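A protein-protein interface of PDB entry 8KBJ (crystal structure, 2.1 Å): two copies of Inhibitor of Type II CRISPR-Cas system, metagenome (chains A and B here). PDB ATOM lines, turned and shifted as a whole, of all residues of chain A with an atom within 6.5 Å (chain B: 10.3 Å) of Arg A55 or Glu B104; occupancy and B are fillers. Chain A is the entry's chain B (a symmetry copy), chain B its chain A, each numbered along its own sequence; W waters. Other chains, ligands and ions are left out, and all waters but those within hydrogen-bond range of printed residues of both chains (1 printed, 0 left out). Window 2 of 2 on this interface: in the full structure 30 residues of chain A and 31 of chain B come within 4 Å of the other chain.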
ATOM      1  N   VAL A  43       7.753 -15.887 -11.776  1.00  0.00           N
ATOM      2  CA  VAL A  43       8.096 -17.264 -11.452  1.00  0.00           C
ATOM      3  C   VAL A  43       9.050 -17.449 -10.251  1.00  0.00           C
ATOM      4  O   VAL A  43       8.836 -18.340  -9.453  1.00  0.00           O
ATOM      5  CB  VAL A  43       8.587 -18.007 -12.696  1.00  0.00           C
ATOM      6  CG1 VAL A  43       8.838 -19.480 -12.419  1.00  0.00           C
ATOM      7  CG2 VAL A  43       7.567 -17.889 -13.813  1.00  0.00           C
ATOM      8  N   PRO A  50       1.082 -18.914  -5.283  1.00  0.00           N
ATOM      9  CA  PRO A  50       1.207 -20.367  -5.243  1.00  0.00           C
ATOM     10  C   PRO A  50       1.947 -20.969  -6.417  1.00  0.00           C
ATOM     11  O   PRO A  50       2.059 -20.368  -7.463  1.00  0.00           O
ATOM     12  CB  PRO A  50      -0.232 -20.833  -5.280  1.00  0.00           C
ATOM     13  CG  PRO A  50      -0.941 -19.804  -6.050  1.00  0.00           C
ATOM     14  CD  PRO A  50      -0.335 -18.542  -5.562  1.00  0.00           C
ATOM     15  N   GLU A  51       2.430 -22.185  -6.232  1.00  0.00           N
ATOM     16  CA  GLU A  51       3.188 -22.850  -7.276  1.00  0.00           C
ATOM     17  C   GLU A  51       2.373 -23.121  -8.487  1.00  0.00           C
ATOM     18  O   GLU A  51       2.875 -23.067  -9.575  1.00  0.00           O
ATOM     19  CB  GLU A  51       3.778 -24.159  -6.763  1.00  0.00           C
ATOM     20  CG  GLU A  51       5.068 -23.998  -5.998  1.00  0.00           C
ATOM     21  CD  GLU A  51       6.219 -23.629  -6.903  1.00  0.00           C
ATOM     22  OE1 GLU A  51       6.226 -24.071  -8.069  1.00  0.00           O
ATOM     23  OE2 GLU A  51       7.116 -22.902  -6.440  1.00  0.00           O
ATOM     24  N   SER A  52       1.104 -23.403  -8.287  1.00  0.00           N
ATOM     25  CA  SER A  52       0.221 -23.694  -9.385  1.00  0.00           C
ATOM     26  C   SER A  52       0.162 -22.483 -10.339  1.00  0.00           C
ATOM     27  O   SER A  52       0.192 -22.662 -11.526  1.00  0.00           O
ATOM     28  CB  SER A  52      -1.157 -24.026  -8.830  1.00  0.00           C
ATOM     29  OG  SER A  52      -1.609 -23.014  -7.956  1.00  0.00           O
ATOM     30  N   PHE A  53       0.088 -21.270  -9.802  1.00  0.00           N
ATOM     31  CA  PHE A  53       0.114 -20.054 -10.626  1.00  0.00           C
ATOM     32  C   PHE A  53       1.454 -19.852 -11.349  1.00  0.00           C
ATOM     33  O   PHE A  53       1.477 -19.508 -12.496  1.00  0.00           O
ATOM     34  CB  PHE A  53      -0.226 -18.821  -9.805  1.00  0.00           C
ATOM     35  CG  PHE A  53      -0.247 -17.554 -10.592  1.00  0.00           C
ATOM     36  CD1 PHE A  53      -1.233 -17.328 -11.528  1.00  0.00           C
ATOM     37  CD2 PHE A  53       0.710 -16.584 -10.387  1.00  0.00           C
ATOM     38  CE1 PHE A  53      -1.255 -16.161 -12.254  1.00  0.00           C
ATOM     39  CE2 PHE A  53       0.691 -15.414 -11.107  1.00  0.00           C
ATOM     40  CZ  PHE A  53      -0.293 -15.201 -12.040  1.00  0.00           C
ATOM     41  N   LYS A  54       2.539 -20.084 -10.634  1.00  0.00           N
ATOM     42  CA  LYS A  54       3.896 -19.950 -11.196  1.00  0.00           C
ATOM     43  C   LYS A  54       4.068 -20.949 -12.314  1.00  0.00           C
ATOM     44  O   LYS A  54       4.572 -20.616 -13.359  1.00  0.00           O
ATOM     45  CB  LYS A  54       4.901 -20.039 -10.071  1.00  0.00           C
ATOM     46  CG  LYS A  54       4.764 -18.855  -9.134  1.00  0.00           C
ATOM     47  CD  LYS A  54       5.878 -18.734  -8.119  1.00  0.00           C
ATOM     48  CE  LYS A  54       5.742 -19.732  -6.996  1.00  0.00           C
ATOM     49  NZ  LYS A  54       6.633 -19.368  -5.865  1.00  0.00           N
ATOM     50  N   ARG A  55       3.557 -22.145 -12.128  1.00  0.00           N
ATOM     51  CA  ARG A  55       3.555 -23.112 -13.186  1.00  0.00           C
ATOM     52  C   ARG A  55       2.701 -22.681 -14.364  1.00  0.00           C
ATOM     53  O   ARG A  55       3.111 -22.849 -15.484  1.00  0.00           O
ATOM     54  CB  ARG A  55       3.136 -24.482 -12.678  1.00  0.00           C
ATOM     55  CG  ARG A  55       4.233 -25.199 -11.909  1.00  0.00           C
ATOM     56  CD  ARG A  55       3.829 -26.594 -11.461  1.00  0.00           C
ATOM     57  NE  ARG A  55       3.310 -26.628 -10.097  1.00  0.00           N
ATOM     58  CZ  ARG A  55       2.064 -26.955  -9.777  1.00  0.00           C
ATOM     59  NH1 ARG A  55       1.684 -26.954  -8.512  1.00  0.00           N
ATOM     60  NH2 ARG A  55       1.200 -27.287 -10.723  1.00  0.00           N
ATOM     61  N   TRP A  56       1.539 -22.099 -14.122  1.00  0.00           N
ATOM     62  CA  TRP A  56       0.738 -21.589 -15.217  1.00  0.00           C
ATOM     63  C   TRP A  56       1.447 -20.522 -16.028  1.00  0.00           C
ATOM     64  O   TRP A  56       1.415 -20.561 -17.257  1.00  0.00           O
ATOM     65  CB  TRP A  56      -0.639 -21.123 -14.758  1.00  0.00           C
ATOM     66  CG  TRP A  56      -1.529 -20.607 -15.852  1.00  0.00           C
ATOM     67  CD1 TRP A  56      -2.447 -21.322 -16.598  1.00  0.00           C
ATOM     68  CD2 TRP A  56      -1.616 -19.236 -16.359  1.00  0.00           C
ATOM     69  NE1 TRP A  56      -3.073 -20.516 -17.502  1.00  0.00           N
ATOM     70  CE2 TRP A  56      -2.619 -19.256 -17.413  1.00  0.00           C
ATOM     71  CE3 TRP A  56      -0.987 -18.048 -16.055  1.00  0.00           C
ATOM     72  CZ2 TRP A  56      -2.956 -18.125 -18.119  1.00  0.00           C
ATOM     73  CZ3 TRP A  56      -1.331 -16.915 -16.777  1.00  0.00           C
ATOM     74  CH2 TRP A  56      -2.293 -16.953 -17.783  1.00  0.00           C
ATOM     75  N   VAL A  57       2.059 -19.557 -15.367  1.00  0.00           N
ATOM     76  CA  VAL A  57       2.775 -18.499 -16.062  1.00  0.00           C
ATOM     77  C   VAL A  57       3.921 -19.095 -16.868  1.00  0.00           C
ATOM     78  O   VAL A  57       4.078 -18.767 -18.022  1.00  0.00           O
ATOM     79  CB  VAL A  57       3.347 -17.475 -15.073  1.00  0.00           C
ATOM     80  CG1 VAL A  57       4.243 -16.461 -15.755  1.00  0.00           C
ATOM     81  CG2 VAL A  57       2.222 -16.776 -14.341  1.00  0.00           C
ATOM     82  N   ALA A  58       4.656 -20.023 -16.279  1.00  0.00           N
ATOM     83  CA  ALA A  58       5.789 -20.648 -16.946  1.00  0.00           C
ATOM     84  C   ALA A  58       5.379 -21.427 -18.168  1.00  0.00           C
ATOM     85  O   ALA A  58       6.127 -21.508 -19.103  1.00  0.00           O
ATOM     86  CB  ALA A  58       6.565 -21.485 -15.970  1.00  0.00           C
ATOM     87  N   ASN A  59       4.255 -22.107 -18.110  1.00  0.00           N
ATOM     88  CA  ASN A  59       3.714 -22.781 -19.267  1.00  0.00           C
ATOM     89  C   ASN A  59       3.165 -21.877 -20.361  1.00  0.00           C
ATOM     90  O   ASN A  59       3.261 -22.223 -21.521  1.00  0.00           O
ATOM     91  CB  ASN A  59       2.668 -23.783 -18.823  1.00  0.00           C
ATOM     92  CG  ASN A  59       3.231 -24.861 -17.914  1.00  0.00           C
ATOM     93  OD1 ASN A  59       4.433 -24.924 -17.669  1.00  0.00           O
ATOM     94  ND2 ASN A  59       2.357 -25.708 -17.396  1.00  0.00           N
ATOM     95  N   ASN A  60       2.544 -20.755 -20.010  1.00  0.00           N
ATOM     96  CA  ASN A  60       1.893 -19.864 -20.984  1.00  0.00           C
ATOM     97  C   ASN A  60       2.657 -18.613 -21.391  1.00  0.00           C
ATOM     98  O   ASN A  60       2.098 -17.744 -22.028  1.00  0.00           O
ATOM     99  CB  ASN A  60       0.494 -19.480 -20.509  1.00  0.00           C
ATOM    100  CG  ASN A  60      -0.444 -20.655 -20.396  1.00  0.00           C
ATOM    101  OD1 ASN A  60      -1.267 -20.882 -21.273  1.00  0.00           O
ATOM    102  ND2 ASN A  60      -0.353 -21.387 -19.300  1.00  0.00           N
ATOM    103  N   MET B   2     -18.151 -28.825  -8.050  1.00  0.00           N
ATOM    104  CA  MET B   2     -18.343 -28.682  -6.622  1.00  0.00           C
ATOM    105  C   MET B   2     -18.984 -27.324  -6.178  1.00  0.00           C
ATOM    106  O   MET B   2     -19.238 -26.422  -6.991  1.00  0.00           O
ATOM    107  CB  MET B   2     -16.983 -28.908  -5.963  1.00  0.00           C
ATOM    108  CG  MET B   2     -15.997 -27.930  -6.416  1.00  0.00           C
ATOM    109  SD  MET B   2     -14.073 -28.125  -6.188  1.00  0.00           S
ATOM    110  CE  MET B   2     -13.713 -29.092  -4.612  1.00  0.00           C
ATOM    111  N   ALA B   7     -14.614 -25.385  -3.301  1.00  0.00           N
ATOM    112  CA  ALA B   7     -13.624 -24.627  -4.041  1.00  0.00           C
ATOM    113  C   ALA B   7     -12.715 -23.851  -3.090  1.00  0.00           C
ATOM    114  O   ALA B   7     -11.518 -23.752  -3.332  1.00  0.00           O
ATOM    115  CB  ALA B   7     -14.299 -23.681  -5.043  1.00  0.00           C
ATOM    116  N   GLU B   9     -11.883 -24.701  -0.018  1.00  0.00           N
ATOM    117  CA  GLU B   9     -10.912 -25.653   0.533  1.00  0.00           C
ATOM    118  C   GLU B   9      -9.819 -25.994  -0.495  1.00  0.00           C
ATOM    119  O   GLU B   9      -8.648 -26.118  -0.145  1.00  0.00           O
ATOM    120  CB  GLU B   9     -11.631 -26.914   1.059  1.00  0.00           C
ATOM    121  CG  GLU B   9     -12.639 -26.628   2.254  1.00  0.00           C
ATOM    122  CD  GLU B   9     -12.033 -25.703   3.373  1.00  0.00           C
ATOM    123  OE1 GLU B   9     -11.169 -26.239   4.119  1.00  0.00           O
ATOM    124  OE2 GLU B   9     -12.427 -24.480   3.549  1.00  0.00           O
ATOM    125  N   SER B  10     -10.165 -26.126  -1.767  1.00  0.00           N
ATOM    126  CA  SER B  10      -9.098 -26.384  -2.744  1.00  0.00           C
ATOM    127  C   SER B  10      -8.168 -25.184  -2.914  1.00  0.00           C
ATOM    128  O   SER B  10      -6.962 -25.369  -3.137  1.00  0.00           O
ATOM    129  CB  SER B  10      -9.692 -26.739  -4.109  1.00  0.00           C
ATOM    130  OG  SER B  10     -10.643 -27.765  -3.952  1.00  0.00           O
ATOM    131  N   LEU B  11      -8.709 -23.955  -2.825  1.00  0.00           N
ATOM    132  CA  LEU B  11      -7.881 -22.751  -2.916  1.00  0.00           C
ATOM    133  C   LEU B  11      -6.903 -22.685  -1.756  1.00  0.00           C
ATOM    134  O   LEU B  11      -5.721 -22.335  -1.946  1.00  0.00           O
ATOM    135  CB  LEU B  11      -8.758 -21.482  -2.936  1.00  0.00           C
ATOM    136  CG  LEU B  11      -9.574 -21.254  -4.212  1.00  0.00           C
ATOM    137  CD1 LEU B  11     -10.779 -20.288  -4.057  1.00  0.00           C
ATOM    138  CD2 LEU B  11      -8.618 -20.679  -5.196  1.00  0.00           C
ATOM    139  N   LYS B  12      -7.370 -23.029  -0.538  1.00  0.00           N
ATOM    140  CA  LYS B  12      -6.451 -23.021   0.603  1.00  0.00           C
ATOM    141  C   LYS B  12      -5.362 -24.090   0.468  1.00  0.00           C
ATOM    142  O   LYS B  12      -4.308 -23.975   1.088  1.00  0.00           O
ATOM    143  CB  LYS B  12      -7.212 -23.203   1.940  1.00  0.00           C
ATOM    144  CG  LYS B  12      -8.204 -22.058   2.313  1.00  0.00           C
ATOM    145  CD  LYS B  12      -9.090 -22.479   3.556  1.00  0.00           C
ATOM    146  CE  LYS B  12     -10.216 -21.448   3.883  1.00  0.00           C
ATOM    147  NZ  LYS B  12     -11.173 -21.938   4.967  1.00  0.00           N
ATOM    148  N   ARG B  13      -5.596 -25.124  -0.310  1.00  0.00           N
ATOM    149  CA  ARG B  13      -4.590 -26.143  -0.575  1.00  0.00           C
ATOM    150  C   ARG B  13      -3.701 -25.791  -1.744  1.00  0.00           C
ATOM    151  O   ARG B  13      -2.873 -26.605  -2.116  1.00  0.00           O
ATOM    152  CB  ARG B  13      -5.276 -27.479  -0.888  1.00  0.00           C
ATOM    153  CG  ARG B  13      -5.771 -28.145   0.356  1.00  0.00           C
ATOM    154  CD  ARG B  13      -6.835 -29.238   0.047  1.00  0.00           C
ATOM    155  NE  ARG B  13      -7.652 -29.371   1.246  1.00  0.00           N
ATOM    156  CZ  ARG B  13      -7.149 -29.735   2.420  1.00  0.00           C
ATOM    157  NH1 ARG B  13      -5.890 -30.097   2.543  1.00  0.00           N
ATOM    158  NH2 ARG B  13      -7.927 -29.726   3.498  1.00  0.00           N
ATOM    159  N   GLY B  14      -3.861 -24.606  -2.331  1.00  0.00           N
ATOM    160  CA  GLY B  14      -2.998 -24.169  -3.395  1.00  0.00           C
ATOM    161  C   GLY B  14      -3.457 -24.424  -4.819  1.00  0.00           C
ATOM    162  O   GLY B  14      -2.664 -24.183  -5.734  1.00  0.00           O
ATOM    163  N   HIS B  15      -4.709 -24.852  -5.051  1.00  0.00           N
ATOM    164  CA  HIS B  15      -5.173 -25.058  -6.425  1.00  0.00           C
ATOM    165  C   HIS B  15      -5.700 -23.773  -7.063  1.00  0.00           C
ATOM    166  O   HIS B  15      -6.077 -22.816  -6.389  1.00  0.00           O
ATOM    167  CB  HIS B  15      -6.318 -26.053  -6.484  1.00  0.00           C
ATOM    168  CG  HIS B  15      -5.925 -27.463  -6.191  1.00  0.00           C
ATOM    169  ND1 HIS B  15      -6.157 -28.054  -4.964  1.00  0.00           N
ATOM    170  CD2 HIS B  15      -5.373 -28.417  -6.976  1.00  0.00           C
ATOM    171  CE1 HIS B  15      -5.750 -29.310  -5.003  1.00  0.00           C
ATOM    172  NE2 HIS B  15      -5.264 -29.554  -6.208  1.00  0.00           N
ATOM    173  N   LEU B  16      -5.789 -23.804  -8.380  1.00  0.00           N
ATOM    174  CA  LEU B  16      -6.549 -22.866  -9.192  1.00  0.00           C
ATOM    175  C   LEU B  16      -7.927 -23.456  -9.470  1.00  0.00           C
ATOM    176  O   LEU B  16      -8.031 -24.640  -9.814  1.00  0.00           O
ATOM    177  CB  LEU B  16      -5.836 -22.608 -10.531  1.00  0.00           C
ATOM    178  CG  LEU B  16      -4.304 -22.433 -10.531  1.00  0.00           C
ATOM    179  CD1 LEU B  16      -3.761 -22.285 -11.971  1.00  0.00           C
ATOM    180  CD2 LEU B  16      -3.941 -21.217  -9.706  1.00  0.00           C
ATOM    181  N   VAL B  17      -8.971 -22.610  -9.377  1.00  0.00           N
ATOM    182  CA  VAL B  17     -10.361 -23.025  -9.585  1.00  0.00           C
ATOM    183  C   VAL B  17     -11.085 -21.979 -10.418  1.00  0.00           C
ATOM    184  O   VAL B  17     -10.653 -20.824 -10.529  1.00  0.00           O
ATOM    185  CB  VAL B  17     -11.130 -23.237  -8.251  1.00  0.00           C
ATOM    186  CG1 VAL B  17     -10.399 -24.241  -7.309  1.00  0.00           C
ATOM    187  CG2 VAL B  17     -11.383 -21.865  -7.512  1.00  0.00           C
ATOM    188  N   ALA B  18     -12.225 -22.385 -10.969  1.00  0.00           N
ATOM    189  CA  ALA B  18     -13.012 -21.538 -11.854  1.00  0.00           C
ATOM    190  C   ALA B  18     -14.444 -22.065 -11.818  1.00  0.00           C
ATOM    191  O   ALA B  18     -14.673 -23.190 -11.391  1.00  0.00           O
ATOM    192  CB  ALA B  18     -12.449 -21.554 -13.285  1.00  0.00           C
ATOM    193  N   GLY B  26     -11.077 -18.653 -20.180  1.00  0.00           N
ATOM    194  CA  GLY B  26      -9.780 -18.964 -19.618  1.00  0.00           C
ATOM    195  C   GLY B  26      -9.380 -18.280 -18.325  1.00  0.00           C
ATOM    196  O   GLY B  26      -8.255 -17.921 -18.157  1.00  0.00           O
ATOM    197  N   MET B  27     -10.318 -18.116 -17.433  1.00  0.00           N
ATOM    198  CA  MET B  27     -10.068 -17.424 -16.199  1.00  0.00           C
ATOM    199  C   MET B  27      -9.971 -18.340 -15.033  1.00  0.00           C
ATOM    200  O   MET B  27     -10.524 -19.414 -15.089  1.00  0.00           O
ATOM    201  CB  MET B  27     -11.234 -16.486 -15.907  1.00  0.00           C
ATOM    202  CG  MET B  27     -11.528 -15.533 -17.043  1.00  0.00           C
ATOM    203  SD  MET B  27     -12.760 -14.119 -16.468  1.00  0.00           S
ATOM    204  CE  MET B  27     -14.311 -15.203 -15.983  1.00  0.00           C
ATOM    205  N   PHE B  28      -9.331 -17.903 -13.969  1.00  0.00           N
ATOM    206  CA  PHE B  28      -9.251 -18.684 -12.761  1.00  0.00           C
ATOM    207  C   PHE B  28      -8.945 -17.838 -11.533  1.00  0.00           C
ATOM    208  O   PHE B  28      -8.502 -16.728 -11.676  1.00  0.00           O
ATOM    209  CB  PHE B  28      -8.229 -19.839 -12.880  1.00  0.00           C
ATOM    210  CG  PHE B  28      -6.818 -19.416 -13.181  1.00  0.00           C
ATOM    211  CD1 PHE B  28      -5.964 -19.002 -12.177  1.00  0.00           C
ATOM    212  CD2 PHE B  28      -6.327 -19.507 -14.464  1.00  0.00           C
ATOM    213  CE1 PHE B  28      -4.662 -18.639 -12.459  1.00  0.00           C
ATOM    214  CE2 PHE B  28      -5.028 -19.156 -14.752  1.00  0.00           C
ATOM    215  CZ  PHE B  28      -4.193 -18.721 -13.750  1.00  0.00           C
ATOM    216  N   ILE B  29      -9.173 -18.367 -10.349  1.00  0.00           N
ATOM    217  CA  ILE B  29      -8.792 -17.640  -9.149  1.00  0.00           C
ATOM    218  C   ILE B  29      -7.838 -18.488  -8.324  1.00  0.00           C
ATOM    219  O   ILE B  29      -7.765 -19.718  -8.463  1.00  0.00           O
ATOM    220  CB  ILE B  29     -10.015 -17.226  -8.284  1.00  0.00           C
ATOM    221  CG1 ILE B  29     -10.871 -18.426  -7.891  1.00  0.00           C
ATOM    222  CG2 ILE B  29     -10.833 -16.171  -9.059  1.00  0.00           C
ATOM    223  CD1 ILE B  29     -12.030 -18.088  -6.922  1.00  0.00           C
ATOM    224  N   PHE B  30      -7.089 -17.806  -7.460  1.00  0.00           N
ATOM    225  CA  PHE B  30      -6.102 -18.493  -6.640  1.00  0.00           C
ATOM    226  C   PHE B  30      -5.918 -17.688  -5.365  1.00  0.00           C
ATOM    227  O   PHE B  30      -6.308 -16.519  -5.271  1.00  0.00           O
ATOM    228  CB  PHE B  30      -4.742 -18.681  -7.363  1.00  0.00           C
ATOM    229  CG  PHE B  30      -4.111 -17.401  -7.830  1.00  0.00           C
ATOM    230  CD1 PHE B  30      -4.465 -16.831  -9.055  1.00  0.00           C
ATOM    231  CD2 PHE B  30      -3.144 -16.774  -7.071  1.00  0.00           C
ATOM    232  CE1 PHE B  30      -3.854 -15.636  -9.497  1.00  0.00           C
ATOM    233  CE2 PHE B  30      -2.529 -15.571  -7.489  1.00  0.00           C
ATOM    234  CZ  PHE B  30      -2.863 -15.000  -8.687  1.00  0.00           C
ATOM    235  N   MET B  31      -5.293 -18.308  -4.395  1.00  0.00           N
ATOM    236  CA  MET B  31      -5.159 -17.678  -3.096  1.00  0.00           C
ATOM    237  C   MET B  31      -3.743 -17.171  -2.895  1.00  0.00           C
ATOM    238  O   MET B  31      -2.801 -17.817  -3.313  1.00  0.00           O
ATOM    239  CB  MET B  31      -5.456 -18.654  -1.971  1.00  0.00           C
ATOM    240  CG  MET B  31      -5.517 -17.928  -0.635  1.00  0.00           C
ATOM    241  SD  MET B  31      -5.908 -19.136   0.763  1.00  0.00           S
ATOM    242  CE  MET B  31      -4.198 -20.079   0.827  1.00  0.00           C
ATOM    243  N   LYS B  78      -6.975 -14.374 -12.346  1.00  0.00           N
ATOM    244  CA  LYS B  78      -6.330 -14.206 -13.624  1.00  0.00           C
ATOM    245  C   LYS B  78      -7.513 -14.003 -14.572  1.00  0.00           C
ATOM    246  O   LYS B  78      -8.231 -14.923 -14.897  1.00  0.00           O
ATOM    247  CB  LYS B  78      -5.460 -15.368 -14.017  1.00  0.00           C
ATOM    248  CG  LYS B  78      -4.745 -15.169 -15.335  1.00  0.00           C
ATOM    249  CD  LYS B  78      -5.383 -16.033 -16.397  1.00  0.00           C
ATOM    250  CE  LYS B  78      -5.351 -15.374 -17.737  1.00  0.00           C
ATOM    251  NZ  LYS B  78      -6.526 -15.819 -18.504  1.00  0.00           N
ATOM    252  N   TRP B 100     -18.282 -25.174  -9.739  1.00  0.00           N
ATOM    253  CA  TRP B 100     -16.871 -24.912  -9.547  1.00  0.00           C
ATOM    254  C   TRP B 100     -16.045 -26.131  -9.955  1.00  0.00           C
ATOM    255  O   TRP B 100     -16.401 -27.265  -9.636  1.00  0.00           O
ATOM    256  CB  TRP B 100     -16.589 -24.589  -8.073  1.00  0.00           C
ATOM    257  CG  TRP B 100     -17.062 -23.232  -7.666  1.00  0.00           C
ATOM    258  CD1 TRP B 100     -18.279 -22.909  -7.133  1.00  0.00           C
ATOM    259  CD2 TRP B 100     -16.339 -21.993  -7.812  1.00  0.00           C
ATOM    260  NE1 TRP B 100     -18.358 -21.524  -6.938  1.00  0.00           N
ATOM    261  CE2 TRP B 100     -17.168 -20.956  -7.315  1.00  0.00           C
ATOM    262  CE3 TRP B 100     -15.085 -21.659  -8.340  1.00  0.00           C
ATOM    263  CZ2 TRP B 100     -16.762 -19.601  -7.303  1.00  0.00           C
ATOM    264  CZ3 TRP B 100     -14.676 -20.303  -8.327  1.00  0.00           C
ATOM    265  CH2 TRP B 100     -15.502 -19.305  -7.800  1.00  0.00           C
ATOM    266  N   VAL B 101     -14.899 -25.880 -10.583  1.00  0.00           N
ATOM    267  CA  VAL B 101     -14.002 -26.936 -11.028  1.00  0.00           C
ATOM    268  C   VAL B 101     -12.581 -26.552 -10.689  1.00  0.00           C
ATOM    269  O   VAL B 101     -12.219 -25.371 -10.683  1.00  0.00           O
ATOM    270  CB  VAL B 101     -14.102 -27.202 -12.554  1.00  0.00           C
ATOM    271  CG1 VAL B 101     -15.417 -27.969 -12.905  1.00  0.00           C
ATOM    272  CG2 VAL B 101     -14.004 -25.886 -13.349  1.00  0.00           C
ATOM    273  N   ILE B 102     -11.758 -27.565 -10.460  1.00  0.00           N
ATOM    274  CA  ILE B 102     -10.308 -27.354 -10.361  1.00  0.00           C
ATOM    275  C   ILE B 102      -9.745 -27.209 -11.763  1.00  0.00           C
ATOM    276  O   ILE B 102     -10.112 -27.951 -12.678  1.00  0.00           O
ATOM    277  CB  ILE B 102      -9.618 -28.497  -9.617  1.00  0.00           C
ATOM    278  CG1 ILE B 102      -9.944 -28.382  -8.128  1.00  0.00           C
ATOM    279  CG2 ILE B 102      -8.084 -28.405  -9.885  1.00  0.00           C
ATOM    280  CD1 ILE B 102      -9.129 -29.297  -7.243  1.00  0.00           C
ATOM    281  N   VAL B 103      -8.898 -26.220 -11.950  1.00  0.00           N
ATOM    282  CA  VAL B 103      -8.354 -25.954 -13.271  1.00  0.00           C
ATOM    283  C   VAL B 103      -6.852 -26.171 -13.257  1.00  0.00           C
ATOM    284  O   VAL B 103      -6.245 -26.418 -14.307  1.00  0.00           O
ATOM    285  CB  VAL B 103      -8.786 -24.540 -13.707  1.00  0.00           C
ATOM    286  CG1 VAL B 103      -7.813 -23.938 -14.636  1.00  0.00           C
ATOM    287  CG2 VAL B 103     -10.243 -24.643 -14.338  1.00  0.00           C
ATOM    288  N   GLU B 104      -6.230 -25.995 -12.099  1.00  0.00           N
ATOM    289  CA  GLU B 104      -4.897 -26.618 -11.913  1.00  0.00           C
ATOM    290  C   GLU B 104      -4.653 -27.031 -10.443  1.00  0.00           C
ATOM    291  O   GLU B 104      -4.771 -26.190  -9.554  1.00  0.00           O
ATOM    292  CB  GLU B 104      -3.754 -25.703 -12.391  1.00  0.00           C
ATOM    293  CG  GLU B 104      -3.122 -26.040 -13.771  1.00  0.00           C
ATOM    294  CD  GLU B 104      -1.798 -25.263 -14.045  1.00  0.00           C
ATOM    295  OE1 GLU B 104      -1.007 -24.964 -13.077  1.00  0.00           O
ATOM    296  OE2 GLU B 104      -1.562 -24.951 -15.250  1.00  0.00           O
ATOM    297  OXT GLU B 104      -4.359 -28.207 -10.116  1.00  0.00           O
HETATM  298  O   HOH W   1       0.038 -24.415  -5.486  1.00  0.00           O
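The side-chain hydroxyl of Ser A52 lies within hydrogen-bond range of the backbone carbonyl oxygen of Gly B14 (2.7 Å).
OE1 of Glu B104 lies within salt-bridge range of NH2 of Arg A55 (3.98 Å).
The side-chain carboxylate (OE1) of Glu B104 sits close to the backbone carbonyl oxygen (O) of Ser A52 (3.0 Å).
O of Leu B16 is in hydrogen-bond range of N of Val B103.
N of Leu B16 lies within hydrogen-bond range of O of Glu B104.
The backbone carbonyl oxygen (O) of Gly B26 sits at hydrogen-bond distance from the side-chain amino group (NZ) of Lys B78 (2.7 Å).
The backbone NH of Lys B78 lies within hydrogen-bond range of the backbone carbonyl oxygen of Phe B28, at 2.9 Å.
The backbone carbonyl oxygen of Arg A55 lies close to the side-chain amide oxygen of Asn A59.
The backbone carbonyl oxygen (O) of Trp A56 is in hydrogen-bond range of the side-chain amide nitrogen (ND2) of Asn A60, at 2.8 Å.
Among the printed residues, pairs that only touch across the chains: Pro A50 with Met B31 (3.4 Å), Ser A52 with Leu B16 (3.4 Å), Trp A56 with Lys B78 (3.4 Å), Trp A56 with Phe B28 (3.6 Å), Pro A50 with Phe B30 (3.6 Å), Phe A53 with Phe B30 (3.7 Å), Phe A53 with Phe B28 (3.8 Å) and Trp A56 with Glu B104 (3.97 Å).
Glu A51 touches none of the printed residues of chain B.
Of the printed residues of chain B, Ser A52 touches Gly B14, Leu B16 and Glu B104.
Of the printed residues of chain B, Phe A53 touches Phe B28 (3.8 Å) and Phe B30 (3.7 Å).
Arg A55 touches just one residue of chain B: Glu B104.
Of the printed residues of chain B, Trp A56 touches Phe B28 (3.6 Å), Lys B78 (3.4 Å) and Glu B104 (3.97 Å).
No residue of chain B comes within 4 Å of Ala A58.
No residue of chain B comes within 4 Å of Asn A59.
Of the printed residues of chain A, Leu B16 touches Ser A52.
Printed residues of chain A within 4 Å of Phe B28: Phe A53 (3.8 Å) and Trp A56 (3.6 Å).
Glu B104 touches just these residues of chain A: Ser A52, Arg A55 and Trp A56.
The nearest printed residue of chain A that does not touch Lys B78 is Phe A53 (4.6 Å).
Printed residues of chain B that touch a printed residue of chain A: Gly B14, Leu B16, Phe B28, Phe B30, Met B31, Lys B78 and Glu B104.
Among the printed residues, 11 pairs touch across the chains.
Among the printed residues, Asp or Glu carboxylates within 4 Å of a Lys or Arg side-chain nitrogen of the other chain: Arg A55 with Glu B104.
No position is printed for both chains.
Of the 11 pairs that touch across the chains among the printed residues, none has its exchanged pair printed and touching as well.
Water W1 lies within hydrogen-bond range of the backbone carbonyl oxygen of Gly B14 (2.7 Å), the backbone NH of Ser A52 (3.2 Å) and the backbone NH of Glu A51 (3.4 Å).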
